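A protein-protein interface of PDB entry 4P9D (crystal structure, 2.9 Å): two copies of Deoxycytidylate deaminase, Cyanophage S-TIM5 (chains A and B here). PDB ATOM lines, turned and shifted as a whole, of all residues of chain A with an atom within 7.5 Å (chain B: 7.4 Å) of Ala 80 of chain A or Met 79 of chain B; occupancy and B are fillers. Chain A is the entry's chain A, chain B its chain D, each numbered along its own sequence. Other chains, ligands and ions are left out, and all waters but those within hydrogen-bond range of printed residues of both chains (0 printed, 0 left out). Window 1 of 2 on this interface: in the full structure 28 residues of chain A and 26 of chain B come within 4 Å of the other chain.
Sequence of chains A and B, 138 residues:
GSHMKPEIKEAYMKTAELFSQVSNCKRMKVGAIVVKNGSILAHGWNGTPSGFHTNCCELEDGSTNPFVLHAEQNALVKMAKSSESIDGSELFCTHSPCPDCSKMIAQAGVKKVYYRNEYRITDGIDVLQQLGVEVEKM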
ATOM      1  N   ALA A  42      -3.935  10.110  20.447  1.00  0.00           N
ATOM      2  CA  ALA A  42      -4.912  10.686  19.530  1.00  0.00           C
ATOM      3  C   ALA A  42      -5.939   9.647  19.099  1.00  0.00           C
ATOM      4  O   ALA A  42      -5.607   8.483  18.883  1.00  0.00           O
ATOM      5  CB  ALA A  42      -4.218  11.274  18.310  1.00  0.00           C
ATOM      6  N   ASN A  74      -7.514  13.214  10.643  1.00  0.00           N
ATOM      7  CA  ASN A  74      -7.837  13.811  11.934  1.00  0.00           C
ATOM      8  C   ASN A  74      -6.899  13.325  13.030  1.00  0.00           C
ATOM      9  O   ASN A  74      -6.554  14.077  13.939  1.00  0.00           O
ATOM     10  CB  ASN A  74      -9.284  13.509  12.321  1.00  0.00           C
ATOM     11  CG  ASN A  74     -10.253  14.554  11.811  1.00  0.00           C
ATOM     12  OD1 ASN A  74      -9.992  15.754  11.897  1.00  0.00           O
ATOM     13  ND2 ASN A  74     -11.385  14.103  11.282  1.00  0.00           N
ATOM     14  N   ALA A  75      -6.493  12.064  12.936  1.00  0.00           N
ATOM     15  CA  ALA A  75      -5.563  11.486  13.898  1.00  0.00           C
ATOM     16  C   ALA A  75      -4.200  12.165  13.810  1.00  0.00           C
ATOM     17  O   ALA A  75      -3.510  12.323  14.815  1.00  0.00           O
ATOM     18  CB  ALA A  75      -5.428   9.989  13.674  1.00  0.00           C
ATOM     19  N   LEU A  76      -3.823  12.570  12.602  1.00  0.00           N
ATOM     20  CA  LEU A  76      -2.539  13.230  12.379  1.00  0.00           C
ATOM     21  C   LEU A  76      -2.609  14.691  12.800  1.00  0.00           C
ATOM     22  O   LEU A  76      -1.715  15.194  13.481  1.00  0.00           O
ATOM     23  CB  LEU A  76      -2.126  13.111  10.907  1.00  0.00           C
ATOM     24  CG  LEU A  76      -0.685  13.421  10.483  1.00  0.00           C
ATOM     25  CD1 LEU A  76      -0.433  12.795   9.132  1.00  0.00           C
ATOM     26  CD2 LEU A  76      -0.392  14.917  10.414  1.00  0.00           C
ATOM     27  N   VAL A  77      -3.670  15.369  12.374  1.00  0.00           N
ATOM     28  CA  VAL A  77      -3.889  16.769  12.717  1.00  0.00           C
ATOM     29  C   VAL A  77      -3.985  16.949  14.231  1.00  0.00           C
ATOM     30  O   VAL A  77      -3.445  17.905  14.791  1.00  0.00           O
ATOM     31  CB  VAL A  77      -5.166  17.308  12.037  1.00  0.00           C
ATOM     32  CG1 VAL A  77      -5.677  18.548  12.745  1.00  0.00           C
ATOM     33  CG2 VAL A  77      -4.905  17.586  10.562  1.00  0.00           C
ATOM     34  N   LYS A  78      -4.654  16.009  14.891  1.00  0.00           N
ATOM     35  CA  LYS A  78      -4.755  16.022  16.344  1.00  0.00           C
ATOM     36  C   LYS A  78      -3.370  15.905  16.972  1.00  0.00           C
ATOM     37  O   LYS A  78      -3.078  16.547  17.981  1.00  0.00           O
ATOM     38  CB  LYS A  78      -5.654  14.883  16.830  1.00  0.00           C
ATOM     39  CG  LYS A  78      -7.136  15.215  16.822  1.00  0.00           C
ATOM     40  CD  LYS A  78      -7.365  16.714  16.717  1.00  0.00           C
ATOM     41  CE  LYS A  78      -8.269  17.053  15.543  1.00  0.00           C
ATOM     42  NZ  LYS A  78      -9.484  16.194  15.511  1.00  0.00           N
ATOM     43  N   MET A  79      -2.519  15.082  16.365  1.00  0.00           N
ATOM     44  CA  MET A  79      -1.151  14.906  16.840  1.00  0.00           C
ATOM     45  C   MET A  79      -0.349  16.191  16.688  1.00  0.00           C
ATOM     46  O   MET A  79       0.560  16.461  17.470  1.00  0.00           O
ATOM     47  CB  MET A  79      -0.461  13.765  16.087  1.00  0.00           C
ATOM     48  CG  MET A  79      -0.780  12.383  16.627  1.00  0.00           C
ATOM     49  SD  MET A  79      -0.826  12.350  18.428  1.00  0.00           S
ATOM     50  CE  MET A  79       0.919  12.445  18.810  1.00  0.00           C
ATOM     51  N   ALA A  80      -0.690  16.977  15.671  1.00  0.00           N
ATOM     52  CA  ALA A  80      -0.032  18.257  15.441  1.00  0.00           C
ATOM     53  C   ALA A  80      -0.394  19.245  16.544  1.00  0.00           C
ATOM     54  O   ALA A  80       0.468  19.958  17.060  1.00  0.00           O
ATOM     55  CB  ALA A  80      -0.411  18.815  14.080  1.00  0.00           C
ATOM     56  N   LYS A  81      -1.672  19.279  16.904  1.00  0.00           N
ATOM     57  CA  LYS A  81      -2.139  20.139  17.983  1.00  0.00           C
ATOM     58  C   LYS A  81      -1.689  19.601  19.335  1.00  0.00           C
ATOM     59  O   LYS A  81      -1.621  20.341  20.316  1.00  0.00           O
ATOM     60  CB  LYS A  81      -3.662  20.267  17.952  1.00  0.00           C
ATOM     61  CG  LYS A  81      -4.215  20.863  16.672  1.00  0.00           C
ATOM     62  CD  LYS A  81      -5.732  20.772  16.638  1.00  0.00           C
ATOM     63  CE  LYS A  81      -6.359  21.671  17.694  1.00  0.00           C
ATOM     64  NZ  LYS A  81      -7.723  22.126  17.307  1.00  0.00           N
ATOM     65  N   SER A  82      -1.386  18.307  19.382  1.00  0.00           N
ATOM     66  CA  SER A  82      -0.944  17.665  20.615  1.00  0.00           C
ATOM     67  C   SER A  82       0.416  18.192  21.059  1.00  0.00           C
ATOM     68  O   SER A  82       1.122  18.843  20.291  1.00  0.00           O
ATOM     69  CB  SER A  82      -0.883  16.145  20.436  1.00  0.00           C
ATOM     70  OG  SER A  82      -0.208  15.528  21.519  1.00  0.00           O
ATOM     71  N   SER A  83       0.773  17.912  22.307  1.00  0.00           N
ATOM     72  CA  SER A  83       2.144  18.302  22.608  1.00  0.00           C
ATOM     73  C   SER A  83       2.994  17.063  22.863  1.00  0.00           C
ATOM     74  O   SER A  83       4.011  17.127  23.552  1.00  0.00           O
ATOM     75  CB  SER A  83       2.187  19.243  23.814  1.00  0.00           C
ATOM     76  OG  SER A  83       1.745  20.544  23.461  1.00  0.00           O
ATOM     77  N   GLU A  84       2.693  16.082  22.016  1.00  0.00           N
ATOM     78  CA  GLU A  84       3.541  14.898  21.952  1.00  0.00           C
ATOM     79  C   GLU A  84       3.818  14.457  20.521  1.00  0.00           C
ATOM     80  O   GLU A  84       3.066  14.775  19.600  1.00  0.00           O
ATOM     81  CB  GLU A  84       2.907  13.748  22.734  1.00  0.00           C
ATOM     82  CG  GLU A  84       3.576  13.479  24.066  1.00  0.00           C
ATOM     83  CD  GLU A  84       4.848  12.670  23.918  1.00  0.00           C
ATOM     84  OE1 GLU A  84       4.809  11.622  23.239  1.00  0.00           O
ATOM     85  OE2 GLU A  84       5.887  13.080  24.474  1.00  0.00           O
ATOM     86  N   SER A  85       4.872  13.661  20.377  1.00  0.00           N
ATOM     87  CA  SER A  85       5.362  13.265  19.066  1.00  0.00           C
ATOM     88  C   SER A  85       4.727  11.963  18.589  1.00  0.00           C
ATOM     89  O   SER A  85       4.684  10.976  19.323  1.00  0.00           O
ATOM     90  CB  SER A  85       6.884  13.123  19.096  1.00  0.00           C
ATOM     91  OG  SER A  85       7.371  12.599  17.875  1.00  0.00           O
ATOM     92  N   ILE A  86       4.233  11.969  17.355  1.00  0.00           N
ATOM     93  CA  ILE A  86       3.675  10.765  16.754  1.00  0.00           C
ATOM     94  C   ILE A  86       4.809   9.891  16.224  1.00  0.00           C
ATOM     95  O   ILE A  86       4.613   8.718  15.905  1.00  0.00           O
ATOM     96  CB  ILE A  86       2.689  11.100  15.614  1.00  0.00           C
ATOM     97  CG1 ILE A  86       1.841   9.876  15.252  1.00  0.00           C
ATOM     98  CG2 ILE A  86       3.434  11.630  14.401  1.00  0.00           C
ATOM     99  CD1 ILE A  86       0.883  10.109  14.107  1.00  0.00           C
ATOM    100  N   VAL B  34       5.984  26.964   9.825  1.00  0.00           N
ATOM    101  CA  VAL B  34       5.057  27.156  10.936  1.00  0.00           C
ATOM    102  C   VAL B  34       5.633  28.127  11.961  1.00  0.00           C
ATOM    103  O   VAL B  34       6.692  27.876  12.537  1.00  0.00           O
ATOM    104  CB  VAL B  34       4.728  25.821  11.632  1.00  0.00           C
ATOM    105  CG1 VAL B  34       3.950  26.066  12.918  1.00  0.00           C
ATOM    106  CG2 VAL B  34       3.957  24.905  10.691  1.00  0.00           C
ATOM    107  N   VAL B  35       4.930  29.233  12.187  1.00  0.00           N
ATOM    108  CA  VAL B  35       5.414  30.279  13.083  1.00  0.00           C
ATOM    109  C   VAL B  35       4.482  30.488  14.273  1.00  0.00           C
ATOM    110  O   VAL B  35       3.264  30.566  14.114  1.00  0.00           O
ATOM    111  CB  VAL B  35       5.581  31.617  12.336  1.00  0.00           C
ATOM    112  CG1 VAL B  35       6.181  32.672  13.255  1.00  0.00           C
ATOM    113  CG2 VAL B  35       6.448  31.430  11.103  1.00  0.00           C
ATOM    114  N   LYS B  36       5.067  30.580  15.465  1.00  0.00           N
ATOM    115  CA  LYS B  36       4.306  30.800  16.689  1.00  0.00           C
ATOM    116  C   LYS B  36       5.213  31.291  17.815  1.00  0.00           C
ATOM    117  O   LYS B  36       6.264  30.703  18.072  1.00  0.00           O
ATOM    118  CB  LYS B  36       3.590  29.517  17.114  1.00  0.00           C
ATOM    119  CG  LYS B  36       2.700  29.679  18.334  1.00  0.00           C
ATOM    120  CD  LYS B  36       1.787  28.476  18.508  1.00  0.00           C
ATOM    121  CE  LYS B  36       1.565  28.158  19.977  1.00  0.00           C
ATOM    122  NZ  LYS B  36       1.137  26.746  20.179  1.00  0.00           N
ATOM    123  N   ILE B  40      10.022  29.527  14.673  1.00  0.00           N
ATOM    124  CA  ILE B  40       9.725  28.736  13.488  1.00  0.00           C
ATOM    125  C   ILE B  40       9.753  27.259  13.859  1.00  0.00           C
ATOM    126  O   ILE B  40      10.813  26.632  13.895  1.00  0.00           O
ATOM    127  CB  ILE B  40      10.718  29.012  12.350  1.00  0.00           C
ATOM    128  CG1 ILE B  40      10.825  30.516  12.093  1.00  0.00           C
ATOM    129  CG2 ILE B  40      10.300  28.275  11.088  1.00  0.00           C
ATOM    130  CD1 ILE B  40      11.806  30.884  11.003  1.00  0.00           C
ATOM    131  N   LEU B  41       8.575  26.713  14.141  1.00  0.00           N
ATOM    132  CA  LEU B  41       8.459  25.362  14.676  1.00  0.00           C
ATOM    133  C   LEU B  41       8.647  24.286  13.612  1.00  0.00           C
ATOM    134  O   LEU B  41       9.038  23.162  13.919  1.00  0.00           O
ATOM    135  CB  LEU B  41       7.100  25.188  15.356  1.00  0.00           C
ATOM    136  CG  LEU B  41       6.850  26.133  16.533  1.00  0.00           C
ATOM    137  CD1 LEU B  41       5.368  26.210  16.866  1.00  0.00           C
ATOM    138  CD2 LEU B  41       7.653  25.685  17.743  1.00  0.00           C
ATOM    139  N   ALA B  42       8.373  24.636  12.360  1.00  0.00           N
ATOM    140  CA  ALA B  42       8.451  23.675  11.267  1.00  0.00           C
ATOM    141  C   ALA B  42       8.708  24.378   9.946  1.00  0.00           C
ATOM    142  O   ALA B  42       8.043  25.356   9.628  1.00  0.00           O
ATOM    143  CB  ALA B  42       7.169  22.865  11.189  1.00  0.00           C
ATOM    144  N   HIS B  43       9.606  23.853   9.157  1.00  0.00           N
ATOM    145  CA  HIS B  43       9.789  24.356   7.828  1.00  0.00           C
ATOM    146  C   HIS B  43       9.814  23.253   6.869  1.00  0.00           C
ATOM    147  O   HIS B  43      10.692  22.475   6.866  1.00  0.00           O
ATOM    148  CB  HIS B  43      11.061  25.117   7.707  1.00  0.00           C
ATOM    149  CG  HIS B  43      12.232  24.422   8.285  1.00  0.00           C
ATOM    150  ND1 HIS B  43      12.836  24.840   9.437  1.00  0.00           N
ATOM    151  CD2 HIS B  43      12.932  23.362   7.858  1.00  0.00           C
ATOM    152  CE1 HIS B  43      13.857  24.064   9.699  1.00  0.00           C
ATOM    153  NE2 HIS B  43      13.936  23.160   8.753  1.00  0.00           N
ATOM    154  N   GLN B  73       2.070  19.540   3.662  1.00  0.00           N
ATOM    155  CA  GLN B  73       1.962  18.224   4.284  1.00  0.00           C
ATOM    156  C   GLN B  73       3.156  17.967   5.195  1.00  0.00           C
ATOM    157  O   GLN B  73       3.003  17.469   6.308  1.00  0.00           O
ATOM    158  CB  GLN B  73       1.859  17.123   3.224  1.00  0.00           C
ATOM    159  CG  GLN B  73       0.560  17.139   2.429  1.00  0.00           C
ATOM    160  CD  GLN B  73       0.438  15.959   1.481  1.00  0.00           C
ATOM    161  OE1 GLN B  73       1.368  15.645   0.739  1.00  0.00           O
ATOM    162  NE2 GLN B  73      -0.715  15.300   1.503  1.00  0.00           N
ATOM    163  N   ASN B  74       4.345  18.319   4.718  1.00  0.00           N
ATOM    164  CA  ASN B  74       5.562  18.166   5.507  1.00  0.00           C
ATOM    165  C   ASN B  74       5.599  19.114   6.701  1.00  0.00           C
ATOM    166  O   ASN B  74       6.054  18.742   7.783  1.00  0.00           O
ATOM    167  CB  ASN B  74       6.794  18.382   4.629  1.00  0.00           C
ATOM    168  CG  ASN B  74       7.197  17.132   3.875  1.00  0.00           C
ATOM    169  OD1 ASN B  74       7.115  16.023   4.402  1.00  0.00           O
ATOM    170  ND2 ASN B  74       7.637  17.305   2.634  1.00  0.00           N
ATOM    171  N   ALA B  75       5.121  20.338   6.497  1.00  0.00           N
ATOM    172  CA  ALA B  75       5.043  21.317   7.575  1.00  0.00           C
ATOM    173  C   ALA B  75       4.071  20.836   8.645  1.00  0.00           C
ATOM    174  O   ALA B  75       4.265  21.078   9.834  1.00  0.00           O
ATOM    175  CB  ALA B  75       4.621  22.674   7.038  1.00  0.00           C
ATOM    176  N   LEU B  76       3.025  20.144   8.204  1.00  0.00           N
ATOM    177  CA  LEU B  76       2.027  19.585   9.103  1.00  0.00           C
ATOM    178  C   LEU B  76       2.559  18.349   9.831  1.00  0.00           C
ATOM    179  O   LEU B  76       2.411  18.221  11.048  1.00  0.00           O
ATOM    180  CB  LEU B  76       0.761  19.226   8.325  1.00  0.00           C
ATOM    181  CG  LEU B  76      -0.552  19.192   9.107  1.00  0.00           C
ATOM    182  CD1 LEU B  76      -0.870  20.549   9.724  1.00  0.00           C
ATOM    183  CD2 LEU B  76      -1.684  18.730   8.208  1.00  0.00           C
ATOM    184  N   VAL B  77       3.175  17.445   9.073  1.00  0.00           N
ATOM    185  CA  VAL B  77       3.678  16.179   9.602  1.00  0.00           C
ATOM    186  C   VAL B  77       4.784  16.374  10.648  1.00  0.00           C
ATOM    187  O   VAL B  77       4.835  15.664  11.651  1.00  0.00           O
ATOM    188  CB  VAL B  77       4.193  15.278   8.442  1.00  0.00           C
ATOM    189  CG1 VAL B  77       5.142  14.204   8.956  1.00  0.00           C
ATOM    190  CG2 VAL B  77       3.025  14.648   7.702  1.00  0.00           C
ATOM    191  N   LYS B  78       5.651  17.360  10.427  1.00  0.00           N
ATOM    192  CA  LYS B  78       6.750  17.629  11.356  1.00  0.00           C
ATOM    193  C   LYS B  78       6.205  18.149  12.689  1.00  0.00           C
ATOM    194  O   LYS B  78       6.789  17.874  13.755  1.00  0.00           O
ATOM    195  CB  LYS B  78       7.750  18.623  10.760  1.00  0.00           C
ATOM    196  CG  LYS B  78       8.347  19.584  11.758  1.00  0.00           C
ATOM    197  CD  LYS B  78       9.545  18.968  12.483  1.00  0.00           C
ATOM    198  CE  LYS B  78      10.397  20.040  13.120  1.00  0.00           C
ATOM    199  NZ  LYS B  78       9.540  20.946  13.953  1.00  0.00           N
ATOM    200  N   MET B  79       5.111  18.909  12.626  1.00  0.00           N
ATOM    201  CA  MET B  79       4.415  19.306  13.829  1.00  0.00           C
ATOM    202  C   MET B  79       3.859  18.085  14.549  1.00  0.00           C
ATOM    203  O   MET B  79       3.809  18.054  15.777  1.00  0.00           O
ATOM    204  CB  MET B  79       3.301  20.283  13.498  1.00  0.00           C
ATOM    205  CG  MET B  79       3.765  21.659  13.033  1.00  0.00           C
ATOM    206  SD  MET B  79       5.065  22.367  14.067  1.00  0.00           S
ATOM    207  CE  MET B  79       4.255  22.469  15.662  1.00  0.00           C
ATOM    208  N   ALA B  80       3.432  17.086  13.782  1.00  0.00           N
ATOM    209  CA  ALA B  80       2.975  15.836  14.367  1.00  0.00           C
ATOM    210  C   ALA B  80       4.150  15.102  15.008  1.00  0.00           C
ATOM    211  O   ALA B  80       3.983  14.392  15.999  1.00  0.00           O
ATOM    212  CB  ALA B  80       2.294  14.965  13.317  1.00  0.00           C
ATOM    213  N   LYS B  81       5.338  15.284  14.439  1.00  0.00           N
ATOM    214  CA  LYS B  81       6.550  14.680  14.981  1.00  0.00           C
ATOM    215  C   LYS B  81       7.132  15.519  16.110  1.00  0.00           C
ATOM    216  O   LYS B  81       8.008  15.067  16.846  1.00  0.00           O
ATOM    217  CB  LYS B  81       7.603  14.498  13.886  1.00  0.00           C
ATOM    218  CG  LYS B  81       7.152  13.650  12.714  1.00  0.00           C
ATOM    219  CD  LYS B  81       8.095  13.803  11.534  1.00  0.00           C
ATOM    220  CE  LYS B  81       9.210  12.772  11.586  1.00  0.00           C
ATOM    221  NZ  LYS B  81      10.208  12.963  10.498  1.00  0.00           N
ATOM    222  N   SER B  82       6.647  16.748  16.236  1.00  0.00           N
ATOM    223  CA  SER B  82       7.174  17.675  17.227  1.00  0.00           C
ATOM    224  C   SER B  82       6.628  17.386  18.618  1.00  0.00           C
ATOM    225  O   SER B  82       5.766  16.528  18.795  1.00  0.00           O
ATOM    226  CB  SER B  82       6.845  19.116  16.831  1.00  0.00           C
ATOM    227  OG  SER B  82       7.340  19.418  15.539  1.00  0.00           O
ATOM    228  N   SER B  83       7.153  18.103  19.605  1.00  0.00           N
ATOM    229  CA  SER B  83       6.572  18.113  20.939  1.00  0.00           C
ATOM    230  C   SER B  83       6.002  19.504  21.183  1.00  0.00           C
ATOM    231  O   SER B  83       5.884  19.960  22.321  1.00  0.00           O
ATOM    232  CB  SER B  83       7.607  17.741  22.002  1.00  0.00           C
ATOM    233  OG  SER B  83       8.508  18.807  22.242  1.00  0.00           O
ATOM    234  N   GLU B  84       5.661  20.173  20.086  1.00  0.00           N
ATOM    235  CA  GLU B  84       5.068  21.504  20.120  1.00  0.00           C
ATOM    236  C   GLU B  84       3.725  21.494  19.398  1.00  0.00           C
ATOM    237  O   GLU B  84       3.494  20.670  18.513  1.00  0.00           O
ATOM    238  CB  GLU B  84       6.008  22.531  19.484  1.00  0.00           C
ATOM    239  CG  GLU B  84       7.201  22.907  20.349  1.00  0.00           C
ATOM    240  CD  GLU B  84       6.808  23.736  21.556  1.00  0.00           C
ATOM    241  OE1 GLU B  84       5.976  24.654  21.402  1.00  0.00           O
ATOM    242  OE2 GLU B  84       7.330  23.470  22.659  1.00  0.00           O
ATOM    243  N   SER B  85       2.842  22.412  19.775  1.00  0.00           N
ATOM    244  CA  SER B  85       1.501  22.453  19.206  1.00  0.00           C
ATOM    245  C   SER B  85       1.400  23.430  18.039  1.00  0.00           C
ATOM    246  O   SER B  85       1.921  24.544  18.101  1.00  0.00           O
ATOM    247  CB  SER B  85       0.478  22.823  20.281  1.00  0.00           C
ATOM    248  OG  SER B  85      -0.837  22.807  19.754  1.00  0.00           O
ATOM    249  N   ILE B  86       0.725  23.002  16.978  1.00  0.00           N
ATOM    250  CA  ILE B  86       0.501  23.853  15.817  1.00  0.00           C
ATOM    251  C   ILE B  86      -0.708  24.752  16.066  1.00  0.00           C
ATOM    252  O   ILE B  86      -0.943  25.717  15.339  1.00  0.00           O
ATOM    253  CB  ILE B  86       0.279  23.021  14.534  1.00  0.00           C
ATOM    254  CG1 ILE B  86       0.443  23.892  13.286  1.00  0.00           C
ATOM    255  CG2 ILE B  86      -1.090  22.359  14.556  1.00  0.00           C
ATOM    256  CD1 ILE B  86       0.314  23.133  11.989  1.00  0.00           C
ATOM    257  N   ASP B  87      -1.468  24.429  17.107  1.00  0.00           N
ATOM    258  CA  ASP B  87      -2.663  25.190  17.453  1.00  0.00           C
ATOM    259  C   ASP B  87      -2.311  26.615  17.870  1.00  0.00           C
ATOM    260  O   ASP B  87      -1.609  26.828  18.858  1.00  0.00           O
ATOM    261  CB  ASP B  87      -3.437  24.490  18.573  1.00  0.00           C
ATOM    262  CG  ASP B  87      -4.738  25.193  18.908  1.00  0.00           C
ATOM    263  OD1 ASP B  87      -5.363  25.760  17.989  1.00  0.00           O
ATOM    264  OD2 ASP B  87      -5.137  25.177  20.092  1.00  0.00           O
ATOM    265  N   SER B  89      -0.834  28.727  15.695  1.00  0.00           N
ATOM    266  CA  SER B  89       0.256  29.163  14.831  1.00  0.00           C
ATOM    267  C   SER B  89      -0.247  29.846  13.564  1.00  0.00           C
ATOM    268  O   SER B  89      -1.429  29.771  13.227  1.00  0.00           O
ATOM    269  CB  SER B  89       1.142  27.975  14.454  1.00  0.00           C
ATOM    270  OG  SER B  89       0.487  27.129  13.525  1.00  0.00           O
ATOM    271  N   LEU B  91       0.850  30.485   9.277  1.00  0.00           N
ATOM    272  CA  LEU B  91       1.537  29.721   8.243  1.00  0.00           C
ATOM    273  C   LEU B  91       2.047  30.597   7.099  1.00  0.00           C
ATOM    274  O   LEU B  91       1.297  31.385   6.523  1.00  0.00           O
ATOM    275  CB  LEU B  91       0.601  28.637   7.703  1.00  0.00           C
ATOM    276  CG  LEU B  91       1.201  27.482   6.906  1.00  0.00           C
ATOM    277  CD1 LEU B  91       1.942  26.538   7.830  1.00  0.00           C
ATOM    278  CD2 LEU B  91       0.105  26.744   6.164  1.00  0.00           C
ATOM    279  N   MET B 104      -6.787  20.359   6.079  1.00  0.00           N
ATOM    280  CA  MET B 104      -6.051  19.917   7.255  1.00  0.00           C
ATOM    281  C   MET B 104      -5.455  21.098   8.020  1.00  0.00           C
ATOM    282  O   MET B 104      -5.263  21.025   9.233  1.00  0.00           O
ATOM    283  CB  MET B 104      -4.946  18.940   6.850  1.00  0.00           C
ATOM    284  CG  MET B 104      -5.437  17.729   6.073  1.00  0.00           C
ATOM    285  SD  MET B 104      -4.146  16.495   5.830  1.00  0.00           S
ATOM    286  CE  MET B 104      -2.978  17.420   4.839  1.00  0.00           C
ATOM    287  N   ALA B 108      -6.180  22.005  11.870  1.00  0.00           N
ATOM    288  CA  ALA B 108      -4.985  22.076  12.702  1.00  0.00           C
ATOM    289  C   ALA B 108      -5.051  23.239  13.685  1.00  0.00           C
ATOM    290  O   ALA B 108      -4.261  23.314  14.625  1.00  0.00           O
ATOM    291  CB  ALA B 108      -3.744  22.192  11.832  1.00  0.00           C
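Met 79 of chain A touches its own counterpart, Met 79 of chain B. Met 79 of chain A touches Ala 80 of chain B, and with the chains exchanged Ala 80 of chain A touches Met 79 of chain B. Ala 80 of chain A touches Ser 85 of chain B, and with the chains exchanged Ser 85 of chain A touches Ala 80 of chain B. Ser 83 of chain B touches its own counterpart, Ser 83 of chain A. Of the 21 pairs that touch across the chains among the printed residues, 16 have their exchanged pair printed and touching as well.
Printed residues of chain B within 4 Å of Ala 80 of chain A: Met 79 (3.9 Å), Glu 84 (3.4 Å), Ser 85 (3.4 Å) and Ile 86 (3.1 Å). Of the printed residues of chain A, Met 79 of chain B touches Met 79 (3.99 Å) and Ala 80 (3.9 Å). Of the printed residues of chain B, Met 79 of chain A touches Met 79 (3.99 Å) and Ala 80 (3.98 Å). Of the printed residues of chain A, Ser 82 of chain B touches Glu 84 and Ser 85. Of the printed residues of chain B, Lys 81 of chain A touches Ser 85 (2.6 Å), Ile 86 (3.9 Å) and Ala 108 (3.2 Å). The nearest printed residue of chain B that does not touch Ala 80 of chain A is Ala 80 of chain B (4.01 Å). The nearest printed residue of chain A that does not touch Lys 81 of chain B is Ile 86 of chain A (4.1 Å).
Of the 14 printed residues of chain A, 10 touch a printed residue of chain B. Printed residues of chain A that touch a printed residue of chain B: Leu 76, Val 77, Met 79, Ala 80, Lys 81, Ser 82, Ser 83, Glu 84, Ser 85 and Ile 86. Of the 26 printed residues of chain B, 10 touch a printed residue of chain A. Among the printed residues, 21 pairs touch across the chains. Among the printed residues, no Asp or Glu carboxylate lies within 4 Å of a Lys or Arg side-chain nitrogen of the other chain.
Among the printed residues, pairs that only touch across the chains: Leu 76 of chain A with Ala 80 of chain B (3.96 Å), Val 77 of chain A with Met 104 of chain B (3.7 Å), Val 77 of chain A with Ala 108 of chain B (3.6 Å), Met 79 of chain A with Met 79 of chain B (3.99 Å), Met 79 of chain A with Ala 80 of chain B (3.98 Å), Ala 80 of chain A with Met 79 of chain B (3.9 Å), Ala 80 of chain A with Ser 85 of chain B (3.4 Å), Lys 81 of chain A with Ile 86 of chain B (3.9 Å), Lys 81 of chain A with Ala 108 of chain B (3.2 Å), Ser 82 of chain A with Ser 85 of chain B (3.8 Å), Ser 83 of chain A with Ser 83 of chain B (3.6 Å), Glu 84 of chain A with Ala 80 of chain B (3.7 Å) and Ser 85 of chain A with Ala 80 of chain B (3.5 Å).
The backbone carbonyl oxygen (O) of Ala 80 of chain A sits at hydrogen-bond distance from the backbone NH (N) of Ile 86 of chain B (3.1 Å). The backbone carbonyl oxygen (O) of Lys 81 of chain A is in hydrogen-bond range of the side-chain hydroxyl (OG) of Ser 85 of chain B (2.6 Å). The backbone carbonyl oxygen (O) of Lys 81 of chain B is in hydrogen-bond range of the side-chain hydroxyl (OG) of Ser 85 of chain A, 2.7 Å away. N of Ser 85 of chain A lies close to O of Ser 82 of chain B (3.4 Å). The backbone NH (N) of Ile 86 of chain A is in hydrogen-bond range of the backbone carbonyl oxygen (O) of Ala 80 of chain B (2.8 Å). O of Ala 80 of chain A lies close to O of Glu 84 of chain B (3.4 Å). The backbone carbonyl oxygen of Ser 82 of chain A sits close to the backbone carbonyl oxygen of Glu 84 of chain B, at 3.5 Å. O of Glu 84 of chain A sits close to O of Ser 82 of chain B, 3.3 Å away.
OG of Ser 82 of chain A is in hydrogen-bond range of N of Glu 84 of chain A (3.0 Å). NZ of Lys 36 of chain B lies within hydrogen-bond range of O of Ser 85 of chain B. The backbone carbonyl oxygen (O) of Lys 78 of chain B sits at hydrogen-bond distance from the side-chain hydroxyl (OG) of Ser 82 of chain B (2.4 Å). OG of Ser 85 of chain B sits at hydrogen-bond distance from N of Asp 87 of chain B (3.2 Å). The backbone carbonyl oxygen (O) of Ile 86 of chain B is in hydrogen-bond range of the side-chain hydroxyl (OG) of Ser 89 of chain B.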
